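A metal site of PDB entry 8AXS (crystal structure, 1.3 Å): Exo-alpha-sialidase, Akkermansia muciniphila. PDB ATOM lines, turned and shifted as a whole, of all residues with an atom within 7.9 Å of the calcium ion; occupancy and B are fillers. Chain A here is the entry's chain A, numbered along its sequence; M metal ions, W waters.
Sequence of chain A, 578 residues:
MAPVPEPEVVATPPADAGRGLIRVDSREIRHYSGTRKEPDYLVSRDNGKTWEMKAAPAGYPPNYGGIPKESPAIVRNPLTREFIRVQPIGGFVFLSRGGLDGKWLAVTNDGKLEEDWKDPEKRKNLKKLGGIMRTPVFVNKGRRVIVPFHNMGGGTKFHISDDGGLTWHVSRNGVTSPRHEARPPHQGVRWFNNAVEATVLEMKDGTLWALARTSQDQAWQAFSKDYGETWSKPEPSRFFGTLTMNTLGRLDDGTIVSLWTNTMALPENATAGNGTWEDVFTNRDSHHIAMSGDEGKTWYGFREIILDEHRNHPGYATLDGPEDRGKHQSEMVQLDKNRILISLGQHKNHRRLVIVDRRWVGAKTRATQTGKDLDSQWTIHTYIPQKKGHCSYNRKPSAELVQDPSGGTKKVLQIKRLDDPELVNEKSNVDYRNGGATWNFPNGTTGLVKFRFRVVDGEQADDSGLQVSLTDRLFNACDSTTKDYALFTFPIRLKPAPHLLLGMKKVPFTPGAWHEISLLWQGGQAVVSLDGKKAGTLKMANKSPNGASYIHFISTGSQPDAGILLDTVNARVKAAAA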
ATOM      1  N   HIS A 180      25.549   4.776 -25.546  1.00  0.00           N
ATOM      2  CA  HIS A 180      26.733   4.041 -25.168  1.00  0.00           C
ATOM      3  C   HIS A 180      26.520   2.547 -25.360  1.00  0.00           C
ATOM      4  O   HIS A 180      25.444   2.010 -25.047  1.00  0.00           O
ATOM      5  CB  HIS A 180      27.026   4.299 -23.692  1.00  0.00           C
ATOM      6  CG  HIS A 180      28.159   3.486 -23.152  1.00  0.00           C
ATOM      7  ND1 HIS A 180      28.011   2.605 -22.101  1.00  0.00           N
ATOM      8  CD2 HIS A 180      29.470   3.458 -23.477  1.00  0.00           C
ATOM      9  CE1 HIS A 180      29.178   2.053 -21.826  1.00  0.00           C
ATOM     10  NE2 HIS A 180      30.082   2.573 -22.618  1.00  0.00           N
ATOM     11  N   HIS A 186      33.427  -2.048 -19.472  1.00  0.00           N
ATOM     12  CA  HIS A 186      32.101  -1.866 -18.911  1.00  0.00           C
ATOM     13  C   HIS A 186      31.376  -3.196 -18.698  1.00  0.00           C
ATOM     14  O   HIS A 186      31.497  -4.139 -19.506  1.00  0.00           O
ATOM     15  CB  HIS A 186      31.233  -0.994 -19.833  1.00  0.00           C
ATOM     16  CG  HIS A 186      31.812   0.357 -20.074  1.00  0.00           C
ATOM     17  ND1 HIS A 186      31.762   1.356 -19.102  1.00  0.00           N
ATOM     18  CD2 HIS A 186      32.530   0.851 -21.101  1.00  0.00           C
ATOM     19  CE1 HIS A 186      32.409   2.402 -19.559  1.00  0.00           C
ATOM     20  NE2 HIS A 186      32.865   2.144 -20.776  1.00  0.00           N
ATOM     21  N   GLY A 188      27.932  -2.723 -18.031  1.00  0.00           N
ATOM     22  CA  GLY A 188      26.605  -2.209 -18.255  1.00  0.00           C
ATOM     23  C   GLY A 188      26.713  -0.935 -19.070  1.00  0.00           C
ATOM     24  O   GLY A 188      27.783  -0.583 -19.552  1.00  0.00           O
ATOM     25  N   VAL A 189      25.561  -0.296 -19.293  1.00  0.00           N
ATOM     26  CA  VAL A 189      25.477   0.887 -20.156  1.00  0.00           C
ATOM     27  C   VAL A 189      25.497   2.165 -19.312  1.00  0.00           C
ATOM     28  O   VAL A 189      24.923   2.247 -18.214  1.00  0.00           O
ATOM     29  CB  VAL A 189      24.251   0.874 -21.098  1.00  0.00           C
ATOM     30  CG1 VAL A 189      24.303  -0.332 -22.073  1.00  0.00           C
ATOM     31  CG2 VAL A 189      22.959   0.902 -20.323  1.00  0.00           C
ATOM     32  N   ARG A 190      26.116   3.173 -19.886  1.00  0.00           N
ATOM     33  CA  ARG A 190      26.046   4.535 -19.335  1.00  0.00           C
ATOM     34  C   ARG A 190      24.657   5.127 -19.530  1.00  0.00           C
ATOM     35  O   ARG A 190      23.936   4.784 -20.469  1.00  0.00           O
ATOM     36  CB  ARG A 190      27.044   5.442 -20.053  1.00  0.00           C
ATOM     37  CG  ARG A 190      28.481   5.132 -19.724  1.00  0.00           C
ATOM     38  CD  ARG A 190      29.401   6.074 -20.407  1.00  0.00           C
ATOM     39  NE  ARG A 190      30.817   5.911 -20.098  1.00  0.00           N
ATOM     40  CZ  ARG A 190      31.810   6.199 -20.924  1.00  0.00           C
ATOM     41  NH1 ARG A 190      31.577   6.685 -22.155  1.00  0.00           N
ATOM     42  NH2 ARG A 190      33.056   5.975 -20.539  1.00  0.00           N
ATOM     43  N   TRP A 191      24.271   6.005 -18.611  1.00  0.00           N
ATOM     44  CA  TRP A 191      23.110   6.870 -18.778  1.00  0.00           C
ATOM     45  C   TRP A 191      23.132   7.512 -20.155  1.00  0.00           C
ATOM     46  O   TRP A 191      24.156   8.101 -20.557  1.00  0.00           O
ATOM     47  CB  TRP A 191      23.207   7.956 -17.687  1.00  0.00           C
ATOM     48  CG  TRP A 191      22.061   8.963 -17.628  1.00  0.00           C
ATOM     49  CD1 TRP A 191      20.768   8.770 -18.049  1.00  0.00           C
ATOM     50  CD2 TRP A 191      22.105  10.267 -17.063  1.00  0.00           C
ATOM     51  NE1 TRP A 191      20.015   9.897 -17.799  1.00  0.00           N
ATOM     52  CE2 TRP A 191      20.824  10.841 -17.213  1.00  0.00           C
ATOM     53  CE3 TRP A 191      23.121  11.027 -16.477  1.00  0.00           C
ATOM     54  CZ2 TRP A 191      20.520  12.115 -16.750  1.00  0.00           C
ATOM     55  CZ3 TRP A 191      22.813  12.293 -16.036  1.00  0.00           C
ATOM     56  CH2 TRP A 191      21.539  12.833 -16.209  1.00  0.00           C
ATOM     57  N   PHE A 192      22.019   7.397 -20.877  1.00  0.00           N
ATOM     58  CA  PHE A 192      21.891   7.951 -22.226  1.00  0.00           C
ATOM     59  C   PHE A 192      21.475   9.414 -22.177  1.00  0.00           C
ATOM     60  O   PHE A 192      20.432   9.755 -21.624  1.00  0.00           O
ATOM     61  CB  PHE A 192      20.879   7.193 -23.062  1.00  0.00           C
ATOM     62  CG  PHE A 192      20.747   7.726 -24.475  1.00  0.00           C
ATOM     63  CD1 PHE A 192      21.856   8.048 -25.209  1.00  0.00           C
ATOM     64  CD2 PHE A 192      19.500   7.930 -25.028  1.00  0.00           C
ATOM     65  CE1 PHE A 192      21.724   8.503 -26.539  1.00  0.00           C
ATOM     66  CE2 PHE A 192      19.367   8.406 -26.352  1.00  0.00           C
ATOM     67  CZ  PHE A 192      20.471   8.713 -27.069  1.00  0.00           C
ATOM     68  N   LEU A 243      28.779  13.059 -19.908  1.00  0.00           N
ATOM     69  CA  LEU A 243      27.637  13.380 -19.041  1.00  0.00           C
ATOM     70  C   LEU A 243      27.944  14.561 -18.098  1.00  0.00           C
ATOM     71  O   LEU A 243      27.491  14.599 -16.957  1.00  0.00           O
ATOM     72  CB  LEU A 243      27.144  12.129 -18.291  1.00  0.00           C
ATOM     73  CG  LEU A 243      26.633  11.026 -19.225  1.00  0.00           C
ATOM     74  CD1 LEU A 243      26.590   9.660 -18.514  1.00  0.00           C
ATOM     75  CD2 LEU A 243      25.297  11.370 -19.853  1.00  0.00           C
ATOM     76  N   ALA A 265      34.999   8.695 -16.514  1.00  0.00           N
ATOM     77  CA  ALA A 265      34.280   7.994 -15.460  1.00  0.00           C
ATOM     78  C   ALA A 265      34.831   6.573 -15.267  1.00  0.00           C
ATOM     79  O   ALA A 265      35.489   6.022 -16.165  1.00  0.00           O
ATOM     80  CB  ALA A 265      32.789   7.878 -15.771  1.00  0.00           C
ATOM     81  N   LEU A 266      34.614   6.010 -14.074  1.00  0.00           N
ATOM     82  CA  LEU A 266      34.929   4.592 -13.905  1.00  0.00           C
ATOM     83  C   LEU A 266      34.060   3.757 -14.858  1.00  0.00           C
ATOM     84  O   LEU A 266      32.926   4.128 -15.197  1.00  0.00           O
ATOM     85  CB  LEU A 266      34.665   4.144 -12.459  1.00  0.00           C
ATOM     86  CG  LEU A 266      35.773   4.514 -11.464  1.00  0.00           C
ATOM     87  CD1 LEU A 266      35.247   4.237 -10.069  1.00  0.00           C
ATOM     88  CD2 LEU A 266      37.028   3.718 -11.690  1.00  0.00           C
ATOM     89  N   PRO A 267      34.572   2.620 -15.307  1.00  0.00           N
ATOM     90  CA  PRO A 267      33.719   1.707 -16.080  1.00  0.00           C
ATOM     91  C   PRO A 267      32.430   1.352 -15.370  1.00  0.00           C
ATOM     92  O   PRO A 267      32.349   1.252 -14.143  1.00  0.00           O
ATOM     93  CB  PRO A 267      34.602   0.451 -16.245  1.00  0.00           C
ATOM     94  CG  PRO A 267      35.990   0.919 -16.054  1.00  0.00           C
ATOM     95  CD  PRO A 267      35.895   2.063 -15.037  1.00  0.00           C
ATOM     96  N   GLU A 268      31.377   1.151 -16.171  1.00  0.00           N
ATOM     97  CA  GLU A 268      30.083   0.775 -15.642  1.00  0.00           C
ATOM     98  C   GLU A 268      30.153  -0.559 -14.926  1.00  0.00           C
ATOM     99  O   GLU A 268      30.827  -1.480 -15.380  1.00  0.00           O
ATOM    100  CB  GLU A 268      29.024   0.716 -16.753  1.00  0.00           C
ATOM    101  CG  GLU A 268      28.755   2.092 -17.380  1.00  0.00           C
ATOM    102  CD  GLU A 268      28.160   3.068 -16.385  1.00  0.00           C
ATOM    103  OE1 GLU A 268      27.388   2.661 -15.484  1.00  0.00           O
ATOM    104  OE2 GLU A 268      28.475   4.276 -16.507  1.00  0.00           O
ATOM    105  N   ASN A 269      29.394  -0.674 -13.823  1.00  0.00           N
ATOM    106  CA  ASN A 269      29.365  -1.890 -13.039  1.00  0.00           C
ATOM    107  C   ASN A 269      28.205  -2.788 -13.442  1.00  0.00           C
ATOM    108  O   ASN A 269      27.472  -2.506 -14.408  1.00  0.00           O
ATOM    109  CB  ASN A 269      29.386  -1.533 -11.565  1.00  0.00           C
ATOM    110  CG  ASN A 269      28.118  -0.867 -11.098  1.00  0.00           C
ATOM    111  OD1 ASN A 269      27.025  -1.160 -11.549  1.00  0.00           O
ATOM    112  ND2 ASN A 269      28.249   0.016 -10.077  1.00  0.00           N
ATOM    113  N   THR A 271      25.437  -3.476 -11.986  1.00  0.00           N
ATOM    114  CA  THR A 271      24.118  -3.000 -11.588  1.00  0.00           C
ATOM    115  C   THR A 271      23.844  -1.583 -12.142  1.00  0.00           C
ATOM    116  O   THR A 271      23.231  -0.749 -11.460  1.00  0.00           O
ATOM    117  CB  THR A 271      23.976  -3.009 -10.055  1.00  0.00           C
ATOM    118  OG1 THR A 271      25.010  -2.204  -9.460  1.00  0.00           O
ATOM    119  CG2 THR A 271      24.042  -4.434  -9.503  1.00  0.00           C
ATOM    120  N   ALA A 272      24.314  -1.292 -13.354  1.00  0.00           N
ATOM    121  CA  ALA A 272      24.291   0.088 -13.879  1.00  0.00           C
ATOM    122  C   ALA A 272      22.941   0.557 -14.359  1.00  0.00           C
ATOM    123  O   ALA A 272      22.775   1.771 -14.600  1.00  0.00           O
ATOM    124  CB  ALA A 272      25.303   0.237 -15.000  1.00  0.00           C
ATOM    125  N   GLY A 273      21.976  -0.356 -14.515  1.00  0.00           N
ATOM    126  CA  GLY A 273      20.667   0.018 -15.034  1.00  0.00           C
ATOM    127  C   GLY A 273      20.594  -0.046 -16.544  1.00  0.00           C
ATOM    128  O   GLY A 273      21.522  -0.455 -17.240  1.00  0.00           O
ATOM    129  N   GLY A 275      20.112   2.494 -18.592  1.00  0.00           N
ATOM    130  CA  GLY A 275      20.549   3.682 -19.267  1.00  0.00           C
ATOM    131  C   GLY A 275      19.539   4.797 -19.313  1.00  0.00           C
ATOM    132  O   GLY A 275      19.887   5.875 -19.785  1.00  0.00           O
ATOM    133  N   TRP A 277      18.333   6.440 -16.673  1.00  0.00           N
ATOM    134  CA  TRP A 277      18.819   7.369 -15.669  1.00  0.00           C
ATOM    135  C   TRP A 277      20.199   6.881 -15.204  1.00  0.00           C
ATOM    136  O   TRP A 277      20.665   5.795 -15.568  1.00  0.00           O
ATOM    137  CB  TRP A 277      17.852   7.486 -14.472  1.00  0.00           C
ATOM    138  CG  TRP A 277      16.498   8.146 -14.816  1.00  0.00           C
ATOM    139  CD1 TRP A 277      15.290   7.527 -14.906  1.00  0.00           C
ATOM    140  CD2 TRP A 277      16.273   9.532 -15.126  1.00  0.00           C
ATOM    141  NE1 TRP A 277      14.316   8.441 -15.243  1.00  0.00           N
ATOM    142  CE2 TRP A 277      14.892   9.677 -15.392  1.00  0.00           C
ATOM    143  CE3 TRP A 277      17.108  10.653 -15.211  1.00  0.00           C
ATOM    144  CZ2 TRP A 277      14.323  10.912 -15.722  1.00  0.00           C
ATOM    145  CZ3 TRP A 277      16.539  11.888 -15.540  1.00  0.00           C
ATOM    146  CH2 TRP A 277      15.165  12.005 -15.793  1.00  0.00           C
ATOM    147  N   GLU A 278      20.855   7.730 -14.449  1.00  0.00           N
ATOM    148  CA  GLU A 278      22.194   7.423 -13.948  1.00  0.00           C
ATOM    149  C   GLU A 278      22.105   6.511 -12.729  1.00  0.00           C
ATOM    150  O   GLU A 278      21.132   6.545 -11.968  1.00  0.00           O
ATOM    151  CB  GLU A 278      22.845   8.749 -13.519  1.00  0.00           C
ATOM    152  CG  GLU A 278      24.278   8.631 -13.128  1.00  0.00           C
ATOM    153  CD  GLU A 278      25.157   7.948 -14.185  1.00  0.00           C
ATOM    154  OE1 GLU A 278      25.691   8.629 -15.087  1.00  0.00           O
ATOM    155  OE2 GLU A 278      25.356   6.696 -14.070  1.00  0.00           O
ATOM    156  N   ASP A 279      23.159   5.706 -12.549  1.00  0.00           N
ATOM    157  CA  ASP A 279      23.350   4.938 -11.321  1.00  0.00           C
ATOM    158  C   ASP A 279      24.253   5.670 -10.323  1.00  0.00           C
ATOM    159  O   ASP A 279      23.880   5.809  -9.156  1.00  0.00           O
ATOM    160  CB  ASP A 279      23.772   3.469 -11.540  1.00  0.00           C
ATOM    161  CG  ASP A 279      25.168   3.302 -12.069  1.00  0.00           C
ATOM    162  OD1 ASP A 279      25.616   4.094 -12.898  1.00  0.00           O
ATOM    163  OD2 ASP A 279      25.880   2.330 -11.645  1.00  0.00           O
ATOM    164  N   VAL A 280      25.395   6.157 -10.755  1.00  0.00           N
ATOM    165  CA  VAL A 280      26.338   6.808  -9.869  1.00  0.00           C
ATOM    166  C   VAL A 280      27.270   7.695 -10.685  1.00  0.00           C
ATOM    167  O   VAL A 280      27.686   7.339 -11.779  1.00  0.00           O
ATOM    168  CB  VAL A 280      27.117   5.750  -9.043  1.00  0.00           C
ATOM    169  CG1 VAL A 280      28.035   4.850  -9.894  1.00  0.00           C
ATOM    170  CG2 VAL A 280      27.903   6.476  -7.903  1.00  0.00           C
ATOM    171  N   PHE A 281      27.623   8.839 -10.120  1.00  0.00           N
ATOM    172  CA  PHE A 281      28.561   9.754 -10.748  1.00  0.00           C
ATOM    173  C   PHE A 281      29.977   9.519 -10.203  1.00  0.00           C
ATOM    174  O   PHE A 281      30.224   9.631  -8.990  1.00  0.00           O
ATOM    175  CB  PHE A 281      28.154  11.202 -10.481  1.00  0.00           C
ATOM    176  CG  PHE A 281      26.906  11.619 -11.142  1.00  0.00           C
ATOM    177  CD1 PHE A 281      26.819  11.638 -12.519  1.00  0.00           C
ATOM    178  CD2 PHE A 281      25.795  11.980 -10.410  1.00  0.00           C
ATOM    179  CE1 PHE A 281      25.675  12.038 -13.149  1.00  0.00           C
ATOM    180  CE2 PHE A 281      24.628  12.399 -11.041  1.00  0.00           C
ATOM    181  CZ  PHE A 281      24.575  12.386 -12.419  1.00  0.00           C
ATOM    182  N   THR A 282      30.929   9.241 -11.099  1.00  0.00           N
ATOM    183  CA  THR A 282      32.318   9.011 -10.686  1.00  0.00           C
ATOM    184  C   THR A 282      33.286   9.922 -11.433  1.00  0.00           C
ATOM    185  O   THR A 282      34.447   9.607 -11.623  1.00  0.00           O
ATOM    186  CB  THR A 282      32.761   7.530 -10.837  1.00  0.00           C
ATOM    187  OG1 THR A 282      32.648   7.120 -12.211  1.00  0.00           O
ATOM    188  CG2 THR A 282      31.877   6.635 -10.004  1.00  0.00           C
HETATM  189 CA    CA M   1      26.556   4.916 -14.961  1.00  0.00          CA
HETATM  190  O   HOH W   1      26.600   6.622 -16.714  1.00  0.00           O
HETATM  191  O   HOH W   2      28.400   5.741 -13.803  1.00  0.00           O
HETATM  192  O   HOH W   3      24.633   3.869 -16.004  1.00  0.00           O
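Along chain A the residues within 4 Å of the calcium ion span positions 268 to 279.
The calcium ion is bound by OE2 of Glu 278 (2.3 Å), water W2 (2.3 Å), OD1 of Asp 279 (2.4 Å), water W3 (2.4 Å), water W1 (2.4 Å), OE1 of Glu 268 (2.5 Å) and OE2 of Glu 268 (2.5 Å).
Water W3 lies within hydrogen-bond range of O of Val 189 (2.8 Å), O of Ala 272 (3.1 Å) and N of Trp 191 (3.4 Å). Water W1 lies within hydrogen-bond range of the side-chain carboxylate (OE1) of Glu 278 (2.7 Å) and the backbone NH (N) of Trp 191 (3.1 Å).
N of Val 280 lies close to OE2 of Glu 278, 3.4 Å away. The backbone NH of Glu 268 is in hydrogen-bond range of a ring nitrogen (ND1) of His 186.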
